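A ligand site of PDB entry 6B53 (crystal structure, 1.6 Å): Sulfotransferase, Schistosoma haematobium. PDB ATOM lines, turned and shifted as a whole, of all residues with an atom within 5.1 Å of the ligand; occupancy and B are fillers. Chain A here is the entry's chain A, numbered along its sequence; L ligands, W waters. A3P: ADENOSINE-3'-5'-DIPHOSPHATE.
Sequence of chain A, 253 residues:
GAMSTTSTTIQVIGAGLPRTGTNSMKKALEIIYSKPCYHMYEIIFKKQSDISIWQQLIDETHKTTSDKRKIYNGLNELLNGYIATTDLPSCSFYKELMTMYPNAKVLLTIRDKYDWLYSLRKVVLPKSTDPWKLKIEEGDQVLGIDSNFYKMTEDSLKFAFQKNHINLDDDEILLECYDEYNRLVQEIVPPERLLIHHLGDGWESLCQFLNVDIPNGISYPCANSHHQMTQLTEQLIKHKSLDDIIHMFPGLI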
ATOM      1  N   LEU A  17      12.270  30.626 -32.667  1.00  0.00           N
ATOM      2  CA  LEU A  17      13.427  30.273 -31.845  1.00  0.00           C
ATOM      3  C   LEU A  17      13.093  29.269 -30.737  1.00  0.00           C
ATOM      4  O   LEU A  17      11.915  29.059 -30.416  1.00  0.00           O
ATOM      5  CB  LEU A  17      14.013  31.549 -31.240  1.00  0.00           C
ATOM      6  CG  LEU A  17      14.643  32.455 -32.300  1.00  0.00           C
ATOM      7  CD1 LEU A  17      14.943  33.820 -31.692  1.00  0.00           C
ATOM      8  CD2 LEU A  17      15.905  31.806 -32.849  1.00  0.00           C
ATOM      9  N   PRO A  18      14.131  28.646 -30.132  1.00  0.00           N
ATOM     10  CA  PRO A  18      13.822  27.761 -29.009  1.00  0.00           C
ATOM     11  C   PRO A  18      13.081  28.486 -27.876  1.00  0.00           C
ATOM     12  O   PRO A  18      13.287  29.678 -27.659  1.00  0.00           O
ATOM     13  CB  PRO A  18      15.213  27.276 -28.547  1.00  0.00           C
ATOM     14  CG  PRO A  18      16.190  28.240 -29.130  1.00  0.00           C
ATOM     15  CD  PRO A  18      15.574  28.695 -30.425  1.00  0.00           C
ATOM     16  N   ARG A  19      12.224  27.719 -27.202  1.00  0.00           N
ATOM     17  CA  ARG A  19      11.427  28.185 -26.068  1.00  0.00           C
ATOM     18  C   ARG A  19      10.335  29.159 -26.500  1.00  0.00           C
ATOM     19  O   ARG A  19       9.898  29.998 -25.714  1.00  0.00           O
ATOM     20  CB  ARG A  19      12.313  28.805 -24.965  1.00  0.00           C
ATOM     21  CG  ARG A  19      13.477  27.915 -24.511  1.00  0.00           C
ATOM     22  CD  ARG A  19      13.026  26.475 -24.264  1.00  0.00           C
ATOM     23  NE  ARG A  19      12.108  26.395 -23.127  1.00  0.00           N
ATOM     24  CZ  ARG A  19      11.489  25.279 -22.748  1.00  0.00           C
ATOM     25  NH1 ARG A  19      11.678  24.149 -23.421  1.00  0.00           N
ATOM     26  NH2 ARG A  19      10.681  25.293 -21.697  1.00  0.00           N
ATOM     27  N   THR A  20       9.851  29.014 -27.731  1.00  0.00           N
ATOM     28  CA  THR A  20       8.718  29.807 -28.206  1.00  0.00           C
ATOM     29  C   THR A  20       7.525  28.918 -28.548  1.00  0.00           C
ATOM     30  O   THR A  20       6.633  29.323 -29.284  1.00  0.00           O
ATOM     31  CB  THR A  20       9.063  30.679 -29.455  1.00  0.00           C
ATOM     32  OG1 THR A  20       9.369  29.830 -30.577  1.00  0.00           O
ATOM     33  CG2 THR A  20      10.238  31.595 -29.188  1.00  0.00           C
ATOM     34  N   GLY A  21       7.505  27.713 -27.998  1.00  0.00           N
ATOM     35  CA  GLY A  21       6.408  26.789 -28.237  1.00  0.00           C
ATOM     36  C   GLY A  21       6.624  25.947 -29.479  1.00  0.00           C
ATOM     37  O   GLY A  21       5.659  25.517 -30.129  1.00  0.00           O
ATOM     38  N   THR A  22       7.881  25.687 -29.822  1.00  0.00           N
ATOM     39  CA  THR A  22       8.173  24.873 -31.007  1.00  0.00           C
ATOM     40  C   THR A  22       7.809  23.395 -30.860  1.00  0.00           C
ATOM     41  O   THR A  22       7.430  22.769 -31.847  1.00  0.00           O
ATOM     42  CB  THR A  22       9.663  24.964 -31.398  1.00  0.00           C
ATOM     43  OG1 THR A  22      10.475  24.415 -30.359  1.00  0.00           O
ATOM     44  CG2 THR A  22      10.053  26.424 -31.643  1.00  0.00           C
ATOM     45  N   ASN A  23       7.924  22.841 -29.652  1.00  0.00           N
ATOM     46  CA  ASN A  23       7.524  21.439 -29.473  1.00  0.00           C
ATOM     47  C   ASN A  23       6.026  21.288 -29.643  1.00  0.00           C
ATOM     48  O   ASN A  23       5.561  20.309 -30.244  1.00  0.00           O
ATOM     49  CB  ASN A  23       7.965  20.901 -28.101  1.00  0.00           C
ATOM     50  CG  ASN A  23       7.909  19.381 -28.028  1.00  0.00           C
ATOM     51  OD1 ASN A  23       7.155  18.809 -27.235  1.00  0.00           O
ATOM     52  ND2 ASN A  23       8.706  18.710 -28.857  1.00  0.00           N
ATOM     53  N   SER A  24       5.261  22.240 -29.122  1.00  0.00           N
ATOM     54  CA  SER A  24       3.810  22.179 -29.243  1.00  0.00           C
ATOM     55  C   SER A  24       3.424  22.352 -30.706  1.00  0.00           C
ATOM     56  O   SER A  24       2.468  21.737 -31.171  1.00  0.00           O
ATOM     57  CB  SER A  24       3.140  23.229 -28.375  1.00  0.00           C
ATOM     58  OG  SER A  24       3.297  22.916 -27.007  1.00  0.00           O
ATOM     59  N   HIS A  39      12.301  18.199 -35.071  1.00  0.00           N
ATOM     60  CA  HIS A  39      12.434  19.082 -33.935  1.00  0.00           C
ATOM     61  C   HIS A  39      13.755  18.770 -33.239  1.00  0.00           C
ATOM     62  O   HIS A  39      14.357  17.724 -33.490  1.00  0.00           O
ATOM     63  CB  HIS A  39      11.241  18.898 -32.982  1.00  0.00           C
ATOM     64  CG  HIS A  39      11.217  19.861 -31.828  1.00  0.00           C
ATOM     65  ND1 HIS A  39      11.835  19.605 -30.637  1.00  0.00           N
ATOM     66  CD2 HIS A  39      10.618  21.069 -31.708  1.00  0.00           C
ATOM     67  CE1 HIS A  39      11.626  20.624 -29.808  1.00  0.00           C
ATOM     68  NE2 HIS A  39      10.887  21.523 -30.439  1.00  0.00           N
ATOM     69  N   TYR A  41      14.064  17.746 -30.369  1.00  0.00           N
ATOM     70  CA  TYR A  41      13.880  16.561 -29.555  1.00  0.00           C
ATOM     71  C   TYR A  41      13.958  15.279 -30.411  1.00  0.00           C
ATOM     72  O   TYR A  41      14.165  14.191 -29.865  1.00  0.00           O
ATOM     73  CB  TYR A  41      12.566  16.633 -28.783  1.00  0.00           C
ATOM     74  CG  TYR A  41      12.596  17.617 -27.625  1.00  0.00           C
ATOM     75  CD1 TYR A  41      13.742  18.392 -27.371  1.00  0.00           C
ATOM     76  CD2 TYR A  41      11.514  17.777 -26.783  1.00  0.00           C
ATOM     77  CE1 TYR A  41      13.778  19.298 -26.307  1.00  0.00           C
ATOM     78  CE2 TYR A  41      11.539  18.667 -25.730  1.00  0.00           C
ATOM     79  CZ  TYR A  41      12.666  19.431 -25.488  1.00  0.00           C
ATOM     80  OH  TYR A  41      12.692  20.320 -24.434  1.00  0.00           O
ATOM     81  N   ASP A  87      12.097  24.472 -34.271  1.00  0.00           N
ATOM     82  CA  ASP A  87      13.171  24.653 -33.261  1.00  0.00           C
ATOM     83  C   ASP A  87      14.560  24.710 -33.892  1.00  0.00           C
ATOM     84  O   ASP A  87      14.733  24.523 -35.101  1.00  0.00           O
ATOM     85  CB  ASP A  87      13.120  23.526 -32.215  1.00  0.00           C
ATOM     86  CG  ASP A  87      13.580  23.973 -30.825  1.00  0.00           C
ATOM     87  OD1 ASP A  87      14.193  25.049 -30.708  1.00  0.00           O
ATOM     88  OD2 ASP A  87      13.314  23.233 -29.848  1.00  0.00           O
ATOM     89  N   ARG A 111       6.821  35.055 -28.679  1.00  0.00           N
ATOM     90  CA  ARG A 111       6.304  35.297 -27.339  1.00  0.00           C
ATOM     91  C   ARG A 111       6.999  36.517 -26.739  1.00  0.00           C
ATOM     92  O   ARG A 111       7.963  37.028 -27.305  1.00  0.00           O
ATOM     93  CB  ARG A 111       6.528  34.091 -26.420  1.00  0.00           C
ATOM     94  CG  ARG A 111       7.984  33.896 -26.031  1.00  0.00           C
ATOM     95  CD  ARG A 111       8.230  32.650 -25.198  1.00  0.00           C
ATOM     96  NE  ARG A 111       7.516  32.603 -23.920  1.00  0.00           N
ATOM     97  CZ  ARG A 111       7.674  31.622 -23.024  1.00  0.00           C
ATOM     98  NH1 ARG A 111       8.520  30.631 -23.282  1.00  0.00           N
ATOM     99  NH2 ARG A 111       6.981  31.624 -21.878  1.00  0.00           N
ATOM    100  N   ASP A 115       9.831  36.610 -21.001  1.00  0.00           N
ATOM    101  CA  ASP A 115       9.432  35.231 -20.722  1.00  0.00           C
ATOM    102  C   ASP A 115      10.338  34.264 -21.490  1.00  0.00           C
ATOM    103  O   ASP A 115      10.738  33.208 -20.975  1.00  0.00           O
ATOM    104  CB  ASP A 115       7.989  34.955 -21.120  1.00  0.00           C
ATOM    105  CG  ASP A 115       6.971  35.730 -20.312  1.00  0.00           C
ATOM    106  OD1 ASP A 115       7.290  36.249 -19.213  1.00  0.00           O
ATOM    107  OD2 ASP A 115       5.814  35.803 -20.783  1.00  0.00           O
ATOM    108  N   SER A 119      12.957  31.458 -19.949  1.00  0.00           N
ATOM    109  CA  SER A 119      12.804  30.054 -20.318  1.00  0.00           C
ATOM    110  C   SER A 119      14.123  29.525 -20.898  1.00  0.00           C
ATOM    111  O   SER A 119      14.593  28.420 -20.585  1.00  0.00           O
ATOM    112  CB  SER A 119      11.654  29.893 -21.317  1.00  0.00           C
ATOM    113  OG  SER A 119      11.347  28.527 -21.553  1.00  0.00           O
ATOM    114  N   LEU A 199       2.312  32.644 -28.571  1.00  0.00           N
ATOM    115  CA  LEU A 199       2.116  31.639 -27.549  1.00  0.00           C
ATOM    116  C   LEU A 199       0.706  31.761 -26.962  1.00  0.00           C
ATOM    117  O   LEU A 199       0.361  32.759 -26.328  1.00  0.00           O
ATOM    118  CB  LEU A 199       3.184  31.773 -26.476  1.00  0.00           C
ATOM    119  CG  LEU A 199       3.649  30.539 -25.701  1.00  0.00           C
ATOM    120  CD1 LEU A 199       4.153  29.426 -26.613  1.00  0.00           C
ATOM    121  CD2 LEU A 199       4.728  30.967 -24.737  1.00  0.00           C
ATOM    122  N   GLY A 200      -0.125  30.750 -27.227  1.00  0.00           N
ATOM    123  CA  GLY A 200      -1.485  30.736 -26.736  1.00  0.00           C
ATOM    124  C   GLY A 200      -2.549  30.961 -27.802  1.00  0.00           C
ATOM    125  O   GLY A 200      -3.738  30.934 -27.494  1.00  0.00           O
ATOM    126  N   TYR A 220      -5.080  21.859 -28.307  1.00  0.00           N
ATOM    127  CA  TYR A 220      -3.781  22.294 -28.811  1.00  0.00           C
ATOM    128  C   TYR A 220      -2.695  21.866 -27.811  1.00  0.00           C
ATOM    129  O   TYR A 220      -2.866  22.038 -26.611  1.00  0.00           O
ATOM    130  CB  TYR A 220      -3.744  23.805 -29.047  1.00  0.00           C
ATOM    131  CG  TYR A 220      -2.499  24.259 -29.760  1.00  0.00           C
ATOM    132  CD1 TYR A 220      -2.427  24.251 -31.152  1.00  0.00           C
ATOM    133  CD2 TYR A 220      -1.389  24.692 -29.054  1.00  0.00           C
ATOM    134  CE1 TYR A 220      -1.289  24.658 -31.803  1.00  0.00           C
ATOM    135  CE2 TYR A 220      -0.235  25.087 -29.703  1.00  0.00           C
ATOM    136  CZ  TYR A 220      -0.193  25.076 -31.078  1.00  0.00           C
ATOM    137  OH  TYR A 220       0.965  25.481 -31.716  1.00  0.00           O
ATOM    138  N   PRO A 221      -1.582  21.315 -28.311  1.00  0.00           N
ATOM    139  CA  PRO A 221      -0.524  20.810 -27.420  1.00  0.00           C
ATOM    140  C   PRO A 221       0.055  21.874 -26.500  1.00  0.00           C
ATOM    141  O   PRO A 221       0.187  23.043 -26.894  1.00  0.00           O
ATOM    142  CB  PRO A 221       0.538  20.293 -28.401  1.00  0.00           C
ATOM    143  CG  PRO A 221      -0.227  19.985 -29.672  1.00  0.00           C
ATOM    144  CD  PRO A 221      -1.312  21.010 -29.734  1.00  0.00           C
ATOM    145  N   CYS A 222       0.432  21.487 -25.286  1.00  0.00           N
ATOM    146  CA  CYS A 222       0.879  22.474 -24.284  1.00  0.00           C
ATOM    147  C   CYS A 222       2.001  22.033 -23.339  1.00  0.00           C
ATOM    148  O   CYS A 222       2.028  22.445 -22.174  1.00  0.00           O
ATOM    149  CB  CYS A 222      -0.323  22.898 -23.422  1.00  0.00           C
ATOM    150  SG  CYS A 222      -1.106  21.534 -22.540  1.00  0.00           S
ATOM    151  N   ALA A 223       2.948  21.231 -23.821  1.00  0.00           N
ATOM    152  CA  ALA A 223       3.996  20.709 -22.950  1.00  0.00           C
ATOM    153  C   ALA A 223       5.340  21.381 -23.243  1.00  0.00           C
ATOM    154  O   ALA A 223       5.406  22.355 -23.994  1.00  0.00           O
ATOM    155  CB  ALA A 223       4.123  19.204 -23.090  1.00  0.00           C
ATOM    156  N   ASN A 224       6.394  20.833 -22.621  1.00  0.00           N
ATOM    157  CA  ASN A 224       7.758  21.362 -22.681  1.00  0.00           C
ATOM    158  C   ASN A 224       7.943  22.661 -21.899  1.00  0.00           C
ATOM    159  O   ASN A 224       8.753  23.510 -22.281  1.00  0.00           O
ATOM    160  CB  ASN A 224       8.233  21.578 -24.125  1.00  0.00           C
ATOM    161  CG  ASN A 224       9.728  21.374 -24.275  1.00  0.00           C
ATOM    162  OD1 ASN A 224      10.361  20.750 -23.421  1.00  0.00           O
ATOM    163  ND2 ASN A 224      10.294  21.903 -25.357  1.00  0.00           N
ATOM    164  N   SER A 225       7.195  22.830 -20.811  1.00  0.00           N
ATOM    165  CA  SER A 225       7.366  24.025 -19.953  1.00  0.00           C
ATOM    166  C   SER A 225       8.697  23.942 -19.190  1.00  0.00           C
ATOM    167  O   SER A 225       9.236  22.850 -19.012  1.00  0.00           O
ATOM    168  CB  SER A 225       6.219  24.131 -18.954  1.00  0.00           C
ATOM    169  OG  SER A 225       6.305  23.104 -17.981  1.00  0.00           O
ATOM    170  N   HIS A 226       9.242  25.064 -18.742  1.00  0.00           N
ATOM    171  CA  HIS A 226      10.528  24.941 -18.042  1.00  0.00           C
ATOM    172  C   HIS A 226      10.348  24.243 -16.686  1.00  0.00           C
ATOM    173  O   HIS A 226      11.301  23.635 -16.191  1.00  0.00           O
ATOM    174  CB  HIS A 226      11.239  26.305 -17.893  1.00  0.00           C
ATOM    175  CG  HIS A 226      10.574  27.275 -16.959  1.00  0.00           C
ATOM    176  ND1 HIS A 226      10.745  27.215 -15.597  1.00  0.00           N
ATOM    177  CD2 HIS A 226       9.794  28.350 -17.203  1.00  0.00           C
ATOM    178  CE1 HIS A 226      10.069  28.211 -15.028  1.00  0.00           C
ATOM    179  NE2 HIS A 226       9.484  28.913 -15.983  1.00  0.00           N
HETATM  180  P1  A3P L   1       8.021  28.140 -20.513  1.00  0.00           P
HETATM  181  O1P A3P L   1       9.400  27.518 -20.386  1.00  0.00           O
HETATM  182  O2P A3P L   1       8.054  29.595 -20.100  1.00  0.00           O
HETATM  183  O3P A3P L   1       7.018  27.342 -19.692  1.00  0.00           O
HETATM  184  P2  A3P L   1       9.790  25.126 -26.901  1.00  0.00           P
HETATM  185  O4P A3P L   1      10.160  25.818 -28.206  1.00  0.00           O
HETATM  186  O5P A3P L   1       8.993  23.877 -27.156  1.00  0.00           O
HETATM  187  O6P A3P L   1      10.994  24.750 -26.082  1.00  0.00           O
HETATM  188  O5' A3P L   1       8.855  26.101 -26.066  1.00  0.00           O
HETATM  189  C5' A3P L   1       8.491  25.778 -24.723  1.00  0.00           C
HETATM  190  C4' A3P L   1       7.759  26.941 -24.121  1.00  0.00           C
HETATM  191  O4' A3P L   1       6.479  27.147 -24.785  1.00  0.00           O
HETATM  192  C3' A3P L   1       7.450  26.763 -22.671  1.00  0.00           C
HETATM  193  O3' A3P L   1       7.543  28.058 -22.040  1.00  0.00           O
HETATM  194  C2' A3P L   1       6.070  26.223 -22.723  1.00  0.00           C
HETATM  195  O2' A3P L   1       5.368  26.317 -21.484  1.00  0.00           O
HETATM  196  C1' A3P L   1       5.459  27.070 -23.781  1.00  0.00           C
HETATM  197  N9  A3P L   1       4.288  26.532 -24.355  1.00  0.00           N
HETATM  198  C8  A3P L   1       4.223  25.443 -25.138  1.00  0.00           C
HETATM  199  N7  A3P L   1       2.956  25.235 -25.531  1.00  0.00           N
HETATM  200  C5  A3P L   1       2.183  26.230 -24.993  1.00  0.00           C
HETATM  201  C6  A3P L   1       0.791  26.548 -25.042  1.00  0.00           C
HETATM  202  N6  A3P L   1      -0.097  25.749 -25.780  1.00  0.00           N
HETATM  203  N1  A3P L   1       0.343  27.635 -24.374  1.00  0.00           N
HETATM  204  C2  A3P L   1       1.182  28.408 -23.690  1.00  0.00           C
HETATM  205  N3  A3P L   1       2.486  28.131 -23.603  1.00  0.00           N
HETATM  206  C4  A3P L   1       3.036  27.067 -24.251  1.00  0.00           C
HETATM  207  O   HOH W   1       6.365  23.638 -26.646  1.00  0.00           O
HETATM  208  O   HOH W   2      13.306  23.839 -27.368  1.00  0.00           O
HETATM  209  O   HOH W   3       6.829  26.692 -16.918  1.00  0.00           O
HETATM  210  O   HOH W   4       9.327  31.812 -19.050  1.00  0.00           O
HETATM  211  O   HOH W   5      -2.583  26.201 -26.005  1.00  0.00           O
HETATM  212  O   HOH W   6      -2.235  28.294 -23.816  1.00  0.00           O
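OG of Ser 119 sits at hydrogen-bond distance from O1P of the ligand.
The backbone NH (N) of Asn 23 is in hydrogen-bond range of an oxygen (O5P) of the ligand, 2.9 Å away.
N of Gly 21 sits at hydrogen-bond distance from O5' of the ligand, at 2.9 Å.
An oxygen (O4P) of the ligand sits at hydrogen-bond distance from the backbone NH (N) of Thr 22 (2.8 Å).
The backbone NH (N) of Arg 19 is in hydrogen-bond range of an oxygen (O4P) of the ligand, 3.0 Å away.
O5P of the ligand lies within hydrogen-bond range of ND2 of Asn 224 (3.0 Å).
NH1 of Arg 19 lies within salt-bridge range of O6P of the ligand (2.8 Å).
The side-chain hydroxyl (OG1) of Thr 22 is in hydrogen-bond range of an oxygen (O4P) of the ligand (2.6 Å).
OG of Ser 24 sits at hydrogen-bond distance from N7 of the ligand.
The guanidinium group of Arg 111 lies within salt-bridge range of an oxygen (O2P) of the ligand, 2.9 Å away.
An oxygen (O1P) of the ligand is in hydrogen-bond range of the backbone NH of His 226 (3.0 Å).
The backbone NH of Thr 20 is in hydrogen-bond range of an oxygen (O4P) of the ligand, at 3.2 Å.
N6 of the ligand sits at hydrogen-bond distance from O of Pro 221, 2.9 Å away.
NH2 of Arg 19 lies within hydrogen-bond range of O of Asn 224.
The side-chain amide oxygen of Asn 224 sits at hydrogen-bond distance from the side-chain hydroxyl of Tyr 41.
The backbone NH of Asn 23 lies within hydrogen-bond range of a ring nitrogen (NE2) of His 39 (3.3 Å).
O of Arg 19 is in hydrogen-bond range of NH1 of Arg 111 (2.9 Å).
The side-chain hydroxyl (OG1) of Thr 20 lies within hydrogen-bond range of the backbone carbonyl oxygen (O) of Leu 17, 2.7 Å away.
OG of Ser 119 lies within hydrogen-bond range of NE of Arg 19.
O of Pro 221 is in hydrogen-bond range of OG of Ser 24, 3.1 Å away.
The side-chain hydroxyl (OG1) of Thr 22 sits at hydrogen-bond distance from a ring nitrogen (NE2) of His 39 (2.9 Å).
Residues that only touch the ligand: Pro 18 (3.97 Å), Leu 199 (3.4 Å), Tyr 220 (3.7 Å), Cys 222 (3.7 Å), Ala 223 (3.5 Å) and Ser 225 (3.3 Å).
Hydrophobic or aromatic side chains within 4 Å of the ligand: Leu 199, Tyr 220 and His 226.
17 residues have an atom within 4 Å of the ligand: Pro 18, Arg 19, Thr 20, Gly 21, Thr 22, Asn 23, Ser 24, Arg 111, Ser 119, Leu 199, Tyr 220, Pro 221, Cys 222, Ala 223, Asn 224, Ser 225 and His 226.
Water W1 lies within hydrogen-bond range of O5P of the ligand, N of Ser 24, O of Ala 223 and N of Asn 23.
Water W4 bridges O2P of the ligand and O of Asp 115.
Water W2 lies within hydrogen-bond range of the side-chain carboxylate (OD2) of Asp 87 (2.6 Å) and an oxygen (O6P) of the ligand (2.8 Å).
Water W3 bridges an oxygen (O3P) of the ligand and the backbone NH of His 226.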
